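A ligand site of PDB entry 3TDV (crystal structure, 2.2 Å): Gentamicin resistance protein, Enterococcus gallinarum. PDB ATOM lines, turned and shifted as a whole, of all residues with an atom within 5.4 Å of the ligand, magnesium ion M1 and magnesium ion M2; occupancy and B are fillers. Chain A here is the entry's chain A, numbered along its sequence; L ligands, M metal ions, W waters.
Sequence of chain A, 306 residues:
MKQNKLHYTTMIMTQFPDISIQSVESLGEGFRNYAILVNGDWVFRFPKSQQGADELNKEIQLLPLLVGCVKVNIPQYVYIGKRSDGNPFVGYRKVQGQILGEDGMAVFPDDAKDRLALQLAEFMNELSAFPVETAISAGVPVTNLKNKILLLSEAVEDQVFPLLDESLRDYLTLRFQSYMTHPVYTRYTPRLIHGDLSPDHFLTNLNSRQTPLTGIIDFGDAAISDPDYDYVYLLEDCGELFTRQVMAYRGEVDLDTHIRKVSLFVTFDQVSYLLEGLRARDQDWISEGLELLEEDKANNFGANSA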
ATOM      1  N   LEU A  27       7.907 -21.532  -9.409  1.00  0.00           N
ATOM      2  CA  LEU A  27       7.814 -22.985  -9.526  1.00  0.00           C
ATOM      3  C   LEU A  27       6.428 -23.518  -9.179  1.00  0.00           C
ATOM      4  O   LEU A  27       5.893 -24.383  -9.862  1.00  0.00           O
ATOM      5  CB  LEU A  27       8.880 -23.685  -8.675  1.00  0.00           C
ATOM      6  CG  LEU A  27       8.699 -25.202  -8.829  1.00  0.00           C
ATOM      7  CD1 LEU A  27       8.768 -25.593 -10.310  1.00  0.00           C
ATOM      8  CD2 LEU A  27       9.699 -26.025  -7.990  1.00  0.00           C
ATOM      9  N   GLY A  28       5.874 -23.007  -8.091  1.00  0.00           N
ATOM     10  CA  GLY A  28       4.572 -23.462  -7.631  1.00  0.00           C
ATOM     11  C   GLY A  28       4.126 -22.713  -6.398  1.00  0.00           C
ATOM     12  O   GLY A  28       4.867 -21.907  -5.827  1.00  0.00           O
ATOM     13  N   GLU A  29       2.894 -22.992  -5.976  1.00  0.00           N
ATOM     14  CA  GLU A  29       2.294 -22.226  -4.906  1.00  0.00           C
ATOM     15  C   GLU A  29       1.119 -22.980  -4.292  1.00  0.00           C
ATOM     16  O   GLU A  29       0.317 -23.592  -4.996  1.00  0.00           O
ATOM     17  CB  GLU A  29       1.813 -20.890  -5.454  1.00  0.00           C
ATOM     18  CG  GLU A  29       1.663 -19.813  -4.403  1.00  0.00           C
ATOM     19  CD  GLU A  29       1.072 -18.538  -4.985  1.00  0.00           C
ATOM     20  OE1 GLU A  29       0.923 -18.495  -6.235  1.00  0.00           O
ATOM     21  OE2 GLU A  29       0.760 -17.598  -4.206  1.00  0.00           O
ATOM     22  N   GLY A  30       1.029 -22.920  -2.962  1.00  0.00           N
ATOM     23  CA  GLY A  30      -0.085 -23.520  -2.262  1.00  0.00           C
ATOM     24  C   GLY A  30      -0.670 -22.521  -1.278  1.00  0.00           C
ATOM     25  O   GLY A  30      -0.488 -21.300  -1.418  1.00  0.00           O
ATOM     26  N   PHE A  31      -1.367 -23.030  -0.261  1.00  0.00           N
ATOM     27  CA  PHE A  31      -1.935 -22.155   0.744  1.00  0.00           C
ATOM     28  C   PHE A  31      -0.877 -21.752   1.756  1.00  0.00           C
ATOM     29  O   PHE A  31      -0.977 -20.694   2.373  1.00  0.00           O
ATOM     30  CB  PHE A  31      -3.114 -22.841   1.443  1.00  0.00           C
ATOM     31  CG  PHE A  31      -4.336 -22.975   0.581  1.00  0.00           C
ATOM     32  CD1 PHE A  31      -4.590 -24.163  -0.099  1.00  0.00           C
ATOM     33  CD2 PHE A  31      -5.236 -21.923   0.457  1.00  0.00           C
ATOM     34  CE1 PHE A  31      -5.725 -24.289  -0.898  1.00  0.00           C
ATOM     35  CE2 PHE A  31      -6.371 -22.048  -0.342  1.00  0.00           C
ATOM     36  CZ  PHE A  31      -6.612 -23.234  -1.021  1.00  0.00           C
ATOM     37  N   ARG A  32       0.136 -22.589   1.933  1.00  0.00           N
ATOM     38  CA  ARG A  32       1.136 -22.328   2.957  1.00  0.00           C
ATOM     39  C   ARG A  32       2.425 -21.744   2.408  1.00  0.00           C
ATOM     40  O   ARG A  32       3.129 -21.006   3.102  1.00  0.00           O
ATOM     41  CB  ARG A  32       1.433 -23.604   3.755  1.00  0.00           C
ATOM     42  CG  ARG A  32       0.207 -24.250   4.350  1.00  0.00           C
ATOM     43  CD  ARG A  32      -0.273 -23.477   5.585  1.00  0.00           C
ATOM     44  NE  ARG A  32      -1.366 -24.158   6.275  1.00  0.00           N
ATOM     45  CZ  ARG A  32      -2.664 -23.939   6.035  1.00  0.00           C
ATOM     46  NH1 ARG A  32      -3.024 -23.031   5.133  1.00  0.00           N
ATOM     47  NH2 ARG A  32      -3.577 -24.613   6.707  1.00  0.00           N
ATOM     48  N   ASN A  33       2.749 -22.056   1.145  1.00  0.00           N
ATOM     49  CA  ASN A  33       4.065 -21.701   0.617  1.00  0.00           C
ATOM     50  C   ASN A  33       4.103 -21.191  -0.806  1.00  0.00           C
ATOM     51  O   ASN A  33       3.193 -21.425  -1.607  1.00  0.00           O
ATOM     52  CB  ASN A  33       5.018 -22.878   0.763  1.00  0.00           C
ATOM     53  CG  ASN A  33       5.260 -23.256   2.204  1.00  0.00           C
ATOM     54  OD1 ASN A  33       6.263 -22.855   2.801  1.00  0.00           O
ATOM     55  ND2 ASN A  33       4.355 -24.058   2.769  1.00  0.00           N
ATOM     56  N   TYR A  34       5.190 -20.479  -1.100  1.00  0.00           N
ATOM     57  CA  TYR A  34       5.505 -20.033  -2.453  1.00  0.00           C
ATOM     58  C   TYR A  34       6.898 -20.505  -2.815  1.00  0.00           C
ATOM     59  O   TYR A  34       7.878 -20.206  -2.103  1.00  0.00           O
ATOM     60  CB  TYR A  34       5.498 -18.511  -2.539  1.00  0.00           C
ATOM     61  CG  TYR A  34       5.486 -18.009  -3.954  1.00  0.00           C
ATOM     62  CD1 TYR A  34       4.292 -17.872  -4.641  1.00  0.00           C
ATOM     63  CD2 TYR A  34       6.657 -17.664  -4.604  1.00  0.00           C
ATOM     64  CE1 TYR A  34       4.253 -17.406  -5.927  1.00  0.00           C
ATOM     65  CE2 TYR A  34       6.639 -17.191  -5.909  1.00  0.00           C
ATOM     66  CZ  TYR A  34       5.423 -17.071  -6.559  1.00  0.00           C
ATOM     67  OH  TYR A  34       5.370 -16.598  -7.865  1.00  0.00           O
ATOM     68  N   ALA A  35       7.005 -21.213  -3.935  1.00  0.00           N
ATOM     69  CA  ALA A  35       8.234 -21.869  -4.309  1.00  0.00           C
ATOM     70  C   ALA A  35       8.768 -21.291  -5.610  1.00  0.00           C
ATOM     71  O   ALA A  35       8.017 -21.110  -6.579  1.00  0.00           O
ATOM     72  CB  ALA A  35       8.010 -23.363  -4.415  1.00  0.00           C
ATOM     73  N   VAL A  43      15.017 -25.546  -5.549  1.00  0.00           N
ATOM     74  CA  VAL A  43      13.793 -24.991  -4.980  1.00  0.00           C
ATOM     75  C   VAL A  43      14.060 -24.203  -3.686  1.00  0.00           C
ATOM     76  O   VAL A  43      14.602 -24.754  -2.709  1.00  0.00           O
ATOM     77  CB  VAL A  43      12.757 -26.103  -4.646  1.00  0.00           C
ATOM     78  CG1 VAL A  43      11.455 -25.488  -4.124  1.00  0.00           C
ATOM     79  CG2 VAL A  43      12.508 -26.953  -5.882  1.00  0.00           C
ATOM     80  N   ARG A  45      11.700 -22.267  -0.947  1.00  0.00           N
ATOM     81  CA  ARG A  45      10.295 -22.324  -0.574  1.00  0.00           C
ATOM     82  C   ARG A  45      10.059 -21.380   0.609  1.00  0.00           C
ATOM     83  O   ARG A  45      10.672 -21.564   1.679  1.00  0.00           O
ATOM     84  CB  ARG A  45       9.985 -23.783  -0.202  1.00  0.00           C
ATOM     85  CG  ARG A  45       8.545 -24.183   0.036  1.00  0.00           C
ATOM     86  CD  ARG A  45       8.528 -25.691   0.279  1.00  0.00           C
ATOM     87  NE  ARG A  45       7.254 -26.299   0.699  1.00  0.00           N
ATOM     88  CZ  ARG A  45       7.022 -26.745   1.938  1.00  0.00           C
ATOM     89  NH1 ARG A  45       7.947 -26.609   2.891  1.00  0.00           N
ATOM     90  NH2 ARG A  45       5.873 -27.333   2.222  1.00  0.00           N
ATOM     91  N   LYS A  48       4.092 -18.444   3.445  1.00  0.00           N
ATOM     92  CA  LYS A  48       3.178 -17.354   3.101  1.00  0.00           C
ATOM     93  C   LYS A  48       2.500 -16.791   4.343  1.00  0.00           C
ATOM     94  O   LYS A  48       1.855 -15.743   4.263  1.00  0.00           O
ATOM     95  CB  LYS A  48       2.096 -17.846   2.108  1.00  0.00           C
ATOM     96  CG  LYS A  48       2.504 -17.736   0.623  1.00  0.00           C
ATOM     97  CD  LYS A  48       1.818 -18.813  -0.238  1.00  0.00           C
ATOM     98  CE  LYS A  48       0.380 -18.438  -0.631  1.00  0.00           C
ATOM     99  NZ  LYS A  48      -0.020 -19.050  -1.952  1.00  0.00           N
ATOM    100  N   GLU A  55       4.593 -24.881  10.039  1.00  0.00           N
ATOM    101  CA  GLU A  55       4.597 -26.185   9.398  1.00  0.00           C
ATOM    102  C   GLU A  55       5.998 -26.520   8.885  1.00  0.00           C
ATOM    103  O   GLU A  55       6.487 -27.617   9.097  1.00  0.00           O
ATOM    104  CB  GLU A  55       3.528 -26.277   8.298  1.00  0.00           C
ATOM    105  CG  GLU A  55       2.105 -26.376   8.843  1.00  0.00           C
ATOM    106  CD  GLU A  55       1.057 -26.198   7.756  1.00  0.00           C
ATOM    107  OE1 GLU A  55       1.429 -26.167   6.560  1.00  0.00           O
ATOM    108  OE2 GLU A  55      -0.134 -26.087   8.099  1.00  0.00           O
ATOM    109  N   TYR A  92      16.110 -26.406  -1.393  1.00  0.00           N
ATOM    110  CA  TYR A  92      16.389 -27.824  -1.626  1.00  0.00           C
ATOM    111  C   TYR A  92      16.545 -28.182  -3.088  1.00  0.00           C
ATOM    112  O   TYR A  92      16.009 -27.501  -3.958  1.00  0.00           O
ATOM    113  CB  TYR A  92      15.375 -28.748  -0.912  1.00  0.00           C
ATOM    114  CG  TYR A  92      13.895 -28.555  -1.247  1.00  0.00           C
ATOM    115  CD1 TYR A  92      13.105 -27.640  -0.541  1.00  0.00           C
ATOM    116  CD2 TYR A  92      13.280 -29.330  -2.224  1.00  0.00           C
ATOM    117  CE1 TYR A  92      11.750 -27.488  -0.830  1.00  0.00           C
ATOM    118  CE2 TYR A  92      11.936 -29.195  -2.522  1.00  0.00           C
ATOM    119  CZ  TYR A  92      11.168 -28.278  -1.827  1.00  0.00           C
ATOM    120  OH  TYR A  92       9.820 -28.167  -2.127  1.00  0.00           O
ATOM    121  N   ARG A  93      17.329 -29.240  -3.335  1.00  0.00           N
ATOM    122  CA  ARG A  93      17.434 -29.815  -4.666  1.00  0.00           C
ATOM    123  C   ARG A  93      16.073 -30.239  -5.164  1.00  0.00           C
ATOM    124  O   ARG A  93      15.361 -31.038  -4.504  1.00  0.00           O
ATOM    125  CB  ARG A  93      18.412 -31.001  -4.686  1.00  0.00           C
ATOM    126  CG  ARG A  93      19.883 -30.621  -4.832  1.00  0.00           C
ATOM    127  CD  ARG A  93      20.332 -30.701  -6.286  1.00  0.00           C
ATOM    128  NE  ARG A  93      21.696 -30.208  -6.483  1.00  0.00           N
ATOM    129  CZ  ARG A  93      22.734 -30.546  -5.716  1.00  0.00           C
ATOM    130  NH1 ARG A  93      22.571 -31.395  -4.703  1.00  0.00           N
ATOM    131  NH2 ARG A  93      23.937 -30.047  -5.969  1.00  0.00           N
ATOM    132  N   LYS A  94      15.692 -29.690  -6.314  1.00  0.00           N
ATOM    133  CA  LYS A  94      14.396 -30.020  -6.896  1.00  0.00           C
ATOM    134  C   LYS A  94      14.236 -31.529  -6.896  1.00  0.00           C
ATOM    135  O   LYS A  94      15.150 -32.273  -7.287  1.00  0.00           O
ATOM    136  CB  LYS A  94      14.265 -29.488  -8.319  1.00  0.00           C
ATOM    137  CG  LYS A  94      12.841 -29.569  -8.865  1.00  0.00           C
ATOM    138  CD  LYS A  94      12.720 -28.943 -10.246  1.00  0.00           C
ATOM    139  CE  LYS A  94      13.346 -29.829 -11.314  1.00  0.00           C
ATOM    140  NZ  LYS A  94      12.917 -29.399 -12.680  1.00  0.00           N
ATOM    141  N   VAL A  95      13.093 -31.994  -6.417  1.00  0.00           N
ATOM    142  CA  VAL A  95      12.735 -33.398  -6.543  1.00  0.00           C
ATOM    143  C   VAL A  95      12.354 -33.636  -8.009  1.00  0.00           C
ATOM    144  O   VAL A  95      11.366 -33.084  -8.507  1.00  0.00           O
ATOM    145  CB  VAL A  95      11.593 -33.750  -5.576  1.00  0.00           C
ATOM    146  CG1 VAL A  95      11.175 -35.214  -5.736  1.00  0.00           C
ATOM    147  CG2 VAL A  95      12.019 -33.430  -4.122  1.00  0.00           C
ATOM    148  N   GLY A  97      11.349 -34.788 -11.896  1.00  0.00           N
ATOM    149  CA  GLY A  97      10.222 -35.419 -12.555  1.00  0.00           C
ATOM    150  C   GLY A  97       9.022 -34.530 -12.807  1.00  0.00           C
ATOM    151  O   GLY A  97       9.067 -33.322 -12.610  1.00  0.00           O
ATOM    152  N   ILE A  99       5.041 -33.481 -12.100  1.00  0.00           N
ATOM    153  CA  ILE A  99       3.967 -33.501 -11.096  1.00  0.00           C
ATOM    154  C   ILE A  99       2.712 -34.167 -11.637  1.00  0.00           C
ATOM    155  O   ILE A  99       2.193 -33.762 -12.685  1.00  0.00           O
ATOM    156  CB  ILE A  99       3.578 -32.063 -10.645  1.00  0.00           C
ATOM    157  CG1 ILE A  99       4.762 -31.336  -9.990  1.00  0.00           C
ATOM    158  CG2 ILE A  99       2.354 -32.100  -9.697  1.00  0.00           C
ATOM    159  CD1 ILE A  99       4.864 -31.494  -8.495  1.00  0.00           C
ATOM    160  N   ASP A 196      -1.033 -34.499   3.505  1.00  0.00           N
ATOM    161  CA  ASP A 196      -1.380 -33.722   2.300  1.00  0.00           C
ATOM    162  C   ASP A 196      -1.021 -34.564   1.083  1.00  0.00           C
ATOM    163  O   ASP A 196      -0.493 -34.078   0.074  1.00  0.00           O
ATOM    164  CB  ASP A 196      -0.605 -32.399   2.256  1.00  0.00           C
ATOM    165  CG  ASP A 196      -1.385 -31.276   1.564  1.00  0.00           C
ATOM    166  OD1 ASP A 196      -2.458 -31.561   0.985  1.00  0.00           O
ATOM    167  OD2 ASP A 196      -0.923 -30.112   1.601  1.00  0.00           O
ATOM    168  N   ASP A 200      -0.796 -33.796  -6.594  1.00  0.00           N
ATOM    169  CA  ASP A 200      -0.043 -32.577  -6.915  1.00  0.00           C
ATOM    170  C   ASP A 200       1.260 -32.520  -6.107  1.00  0.00           C
ATOM    171  O   ASP A 200       2.011 -31.565  -6.209  1.00  0.00           O
ATOM    172  CB  ASP A 200      -0.897 -31.363  -6.650  1.00  0.00           C
ATOM    173  CG  ASP A 200      -1.566 -31.426  -5.301  1.00  0.00           C
ATOM    174  OD1 ASP A 200      -0.903 -31.873  -4.332  1.00  0.00           O
ATOM    175  OD2 ASP A 200      -2.774 -31.068  -5.197  1.00  0.00           O
ATOM    176  N   HIS A 201       1.493 -33.538  -5.279  1.00  0.00           N
ATOM    177  CA  HIS A 201       2.769 -33.708  -4.576  1.00  0.00           C
ATOM    178  C   HIS A 201       3.457 -34.996  -5.021  1.00  0.00           C
ATOM    179  O   HIS A 201       4.440 -35.436  -4.415  1.00  0.00           O
ATOM    180  CB  HIS A 201       2.594 -33.684  -3.038  1.00  0.00           C
ATOM    181  CG  HIS A 201       2.009 -32.412  -2.510  1.00  0.00           C
ATOM    182  ND1 HIS A 201       0.940 -32.398  -1.624  1.00  0.00           N
ATOM    183  CD2 HIS A 201       2.317 -31.114  -2.743  1.00  0.00           C
ATOM    184  CE1 HIS A 201       0.639 -31.148  -1.336  1.00  0.00           C
ATOM    185  NE2 HIS A 201       1.457 -30.339  -1.990  1.00  0.00           N
ATOM    186  N   LEU A 203       5.785 -36.703  -7.724  1.00  0.00           N
ATOM    187  CA  LEU A 203       6.732 -36.501  -8.821  1.00  0.00           C
ATOM    188  C   LEU A 203       6.949 -37.820  -9.562  1.00  0.00           C
ATOM    189  O   LEU A 203       7.414 -38.802  -8.975  1.00  0.00           O
ATOM    190  CB  LEU A 203       8.051 -35.971  -8.277  1.00  0.00           C
ATOM    191  CG  LEU A 203       8.009 -34.458  -8.126  1.00  0.00           C
ATOM    192  CD1 LEU A 203       7.434 -33.834  -9.407  1.00  0.00           C
ATOM    193  CD2 LEU A 203       7.198 -34.045  -6.900  1.00  0.00           C
ATOM    194  N   ILE A 217       6.559 -34.519  -2.076  1.00  0.00           N
ATOM    195  CA  ILE A 217       6.901 -33.215  -1.526  1.00  0.00           C
ATOM    196  C   ILE A 217       5.830 -32.734  -0.549  1.00  0.00           C
ATOM    197  O   ILE A 217       4.826 -33.430  -0.326  1.00  0.00           O
ATOM    198  CB  ILE A 217       7.023 -32.147  -2.622  1.00  0.00           C
ATOM    199  CG1 ILE A 217       5.751 -32.146  -3.477  1.00  0.00           C
ATOM    200  CG2 ILE A 217       8.268 -32.385  -3.484  1.00  0.00           C
ATOM    201  CD1 ILE A 217       5.683 -31.014  -4.493  1.00  0.00           C
ATOM    202  N   ASP A 218       6.053 -31.537  -0.014  1.00  0.00           N
ATOM    203  CA  ASP A 218       5.095 -30.902   0.878  1.00  0.00           C
ATOM    204  C   ASP A 218       4.703 -31.765   2.065  1.00  0.00           C
ATOM    205  O   ASP A 218       3.601 -32.316   2.095  1.00  0.00           O
ATOM    206  CB  ASP A 218       3.815 -30.465   0.153  1.00  0.00           C
ATOM    207  CG  ASP A 218       2.980 -29.492   1.017  1.00  0.00           C
ATOM    208  OD1 ASP A 218       3.409 -29.242   2.169  1.00  0.00           O
ATOM    209  OD2 ASP A 218       1.935 -28.974   0.557  1.00  0.00           O
ATOM    210  N   GLY A 220       4.118 -30.516   4.955  1.00  0.00           N
ATOM    211  CA  GLY A 220       3.650 -29.524   5.935  1.00  0.00           C
ATOM    212  C   GLY A 220       2.572 -30.012   6.905  1.00  0.00           C
ATOM    213  O   GLY A 220       2.489 -29.566   8.062  1.00  0.00           O
ATOM    214  N   ASP A 221       1.741 -30.963   6.470  1.00  0.00           N
ATOM    215  CA  ASP A 221       0.641 -31.416   7.311  1.00  0.00           C
ATOM    216  C   ASP A 221       0.982 -32.700   8.037  1.00  0.00           C
ATOM    217  O   ASP A 221       0.091 -33.375   8.559  1.00  0.00           O
ATOM    218  CB  ASP A 221      -0.618 -31.641   6.467  1.00  0.00           C
ATOM    219  CG  ASP A 221      -1.310 -30.351   6.099  1.00  0.00           C
ATOM    220  OD1 ASP A 221      -1.694 -29.587   7.019  1.00  0.00           O
ATOM    221  OD2 ASP A 221      -1.459 -30.099   4.875  1.00  0.00           O
HETATM  222  P1  LIG L   1       2.137 -25.583  -0.037  1.00  0.00           P
HETATM  223  O1  LIG L   1       1.787 -24.155   0.328  1.00  0.00           O
HETATM  224  O2  LIG L   1       0.989 -26.094  -0.903  1.00  0.00           O
HETATM  225  O3  LIG L   1       2.320 -26.401   1.225  1.00  0.00           O
HETATM  226  O4  LIG L   1       3.514 -25.566  -0.892  1.00  0.00           O
HETATM  227  P2  LIG L   1       4.195 -26.877  -1.534  1.00  0.00           P
HETATM  228  O5  LIG L   1       5.276 -27.471  -0.647  1.00  0.00           O
HETATM  229  O6  LIG L   1       3.225 -27.944  -1.989  1.00  0.00           O
HETATM  230  O7  LIG L   1       4.838 -26.246  -2.862  1.00  0.00           O
HETATM  231  C1  LIG L   1       3.908 -25.548  -3.702  1.00  0.00           C
HETATM  232  C2  LIG L   1       4.093 -26.021  -5.126  1.00  0.00           C
HETATM  233  O8  LIG L   1       5.443 -25.803  -5.558  1.00  0.00           O
HETATM  234  C3  LIG L   1       3.890 -27.526  -5.295  1.00  0.00           C
HETATM  235  O9  LIG L   1       2.494 -27.874  -5.383  1.00  0.00           O
HETATM  236  C4  LIG L   1       4.662 -27.797  -6.568  1.00  0.00           C
HETATM  237  O10 LIG L   1       3.919 -27.413  -7.733  1.00  0.00           O
HETATM  238  C5  LIG L   1       5.841 -26.860  -6.449  1.00  0.00           C
HETATM  239  N1  LIG L   1       7.032 -27.605  -5.943  1.00  0.00           N
HETATM  240  C6  LIG L   1       7.562 -27.599  -4.699  1.00  0.00           C
HETATM  241  N2  LIG L   1       8.632 -28.436  -4.601  1.00  0.00           N
HETATM  242  C7  LIG L   1       8.805 -29.010  -5.806  1.00  0.00           C
HETATM  243  C8  LIG L   1       9.759 -29.962  -6.428  1.00  0.00           C
HETATM  244  O11 LIG L   1      10.702 -30.460  -5.763  1.00  0.00           O
HETATM  245  N3  LIG L   1       9.583 -30.279  -7.720  1.00  0.00           N
HETATM  246  C9  LIG L   1       8.585 -29.746  -8.469  1.00  0.00           C
HETATM  247  N4  LIG L   1       8.452 -30.105  -9.773  1.00  0.00           N
HETATM  248  N5  LIG L   1       7.687 -28.857  -7.963  1.00  0.00           N
HETATM  249  C10 LIG L   1       7.742 -28.457  -6.671  1.00  0.00           C
HETATM  250 MG    MG M   1       1.273 -28.243  -1.284  1.00  0.00          MG
HETATM  251 MG    MG M   2       1.991 -27.677   2.732  1.00  0.00          MG
HETATM  252  O   HOH W   1       6.745 -28.600 -11.562  1.00  0.00           O
HETATM  253  O   HOH W   2       1.695 -29.175  -7.518  1.00  0.00           O
HETATM  254  O   HOH W   3      -0.686 -28.644  -0.636  1.00  0.00           O
HETATM  255  O   HOH W   4       0.263 -27.767  -3.052  1.00  0.00           O
HETATM  256  O   HOH W   5      10.683 -31.645 -10.856  1.00  0.00           O
HETATM  257  O   HOH W   6       0.067 -26.818   2.734  1.00  0.00           O
HETATM  258  O   HOH W   7       0.775 -29.374   3.045  1.00  0.00           O
HETATM  259  O   HOH W   8       7.425 -28.951  -0.561  1.00  0.00           O
HETATM  260  O   HOH W   9       2.975 -26.742   4.191  1.00  0.00           O
HETATM  261  O   HOH W  10      -1.281 -25.674   0.239  1.00  0.00           O
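Magnesium ion M1 is bound by OD2 of Asp 218, water W4, O6 of the ligand, water W3, O2 of the ligand and NE2 of His 201.
OD1 of Asp 218 sits close to NH2 of Arg 45 (3.1 Å). The side-chain carboxylate (OD1) of Asp 218 lies close to the backbone NH (N) of Gly 220 (3.1 Å). ND1 of His 201 sits at hydrogen-bond distance from OD1 of Asp 200. O of His 201 sits at hydrogen-bond distance from N of Ile 217 (3.3 Å). A ring nitrogen (ND1) of His 201 is in hydrogen-bond range of the backbone carbonyl oxygen of Asp 196, at 2.8 Å. O of Val 43 lies within hydrogen-bond range of N of Tyr 92, 2.6 Å away. OE2 of Glu 29 lies within salt-bridge range of NZ of Lys 48 (2.8 Å). O of Ala 35 sits at hydrogen-bond distance from N of Leu 27, 2.9 Å away.
Magnesium ion M2 is bound by water W9 (2.0 Å), O3 of the ligand (2.0 Å), water W6 (2.1 Å), water W7 (2.1 Å), OD1 of Asp 218 (2.2 Å) and OD2 of Asp 218 (2.5 Å). Magnesium ion M2 has six donor atoms within binding distance.
Residues that only touch magnesium ion M2: Arg 45 and Asp 196. Within 4 Å of magnesium ion M2: Arg 45, Asp 196 and Asp 218.
Two residues have an atom within 4 Å of magnesium ion M1: His 201 and Asp 218. Along chain A the residues within 4 Å of magnesium ion M1 span positions 201 to 218.
Merely in contact with the ligand: Leu 27, Gly 28, Glu 29, Gly 30, Ala 35, Val 43, Lys 94, Ile 99, Asp 200, Leu 203 and Ile 217. Hydrophobic or aromatic side chains that line the ligand: Leu 27, Ala 35, Val 43, Tyr 92, Val 95, Ile 99, His 201, Leu 203 and Ile 217. Within 4 Å of the ligand: Leu 27, Gly 28, Glu 29, Gly 30, Phe 31, Arg 32, Asn 33, Ala 35, Val 43, Arg 45, Tyr 92, Lys 94, Val 95, Ile 99, Asp 200, His 201, Leu 203, Ile 217 and Asp 218. Along chain A the residues within 4 Å of the ligand span positions 27 to 218.
Water W9 lies within hydrogen-bond range of OE1 of Glu 55 (2.9 Å) and ND2 of Asn 33 (3.3 Å). Water W10 bridges N of Phe 31 (2.7 Å) and O1 of the ligand (3.4 Å). Water W8 lies within hydrogen-bond range of an oxygen (O5) of the ligand (2.6 Å), the guanidinium group of Arg 45 (2.9 Å), the side-chain hydroxyl of Tyr 92 (3.0 Å) and the backbone NH of Asp 218 (3.0 Å). Water W2 lies within hydrogen-bond range of an oxygen (O9) of the ligand (2.6 Å) and the backbone carbonyl oxygen (O) of Asp 200 (2.7 Å). Water W5 lies within hydrogen-bond range of O of Val 95 (2.8 Å), O of Gly 97 (2.9 Å) and N4 of the ligand (2.9 Å).
N of Asn 33 sits at hydrogen-bond distance from O1 of the ligand (2.4 Å). O3 of the ligand lies close to ND2 of Asn 33 (3.5 Å). O5 of the ligand is in salt-bridge range of NE of Arg 45, 2.7 Å away. A nitrogen (N2) of the ligand lies within hydrogen-bond range of the side-chain hydroxyl (OH) of Tyr 92. The backbone NH (N) of Arg 32 sits at hydrogen-bond distance from an oxygen (O1) of the ligand (2.8 Å). The backbone NH (N) of Val 95 sits at hydrogen-bond distance from an oxygen (O11) of the ligand. The backbone carbonyl oxygen (O) of Val 95 sits at hydrogen-bond distance from a nitrogen (N3) of the ligand, 3.4 Å away. The backbone NH of Phe 31 lies within hydrogen-bond range of an oxygen (O1) of the ligand (3.4 Å).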
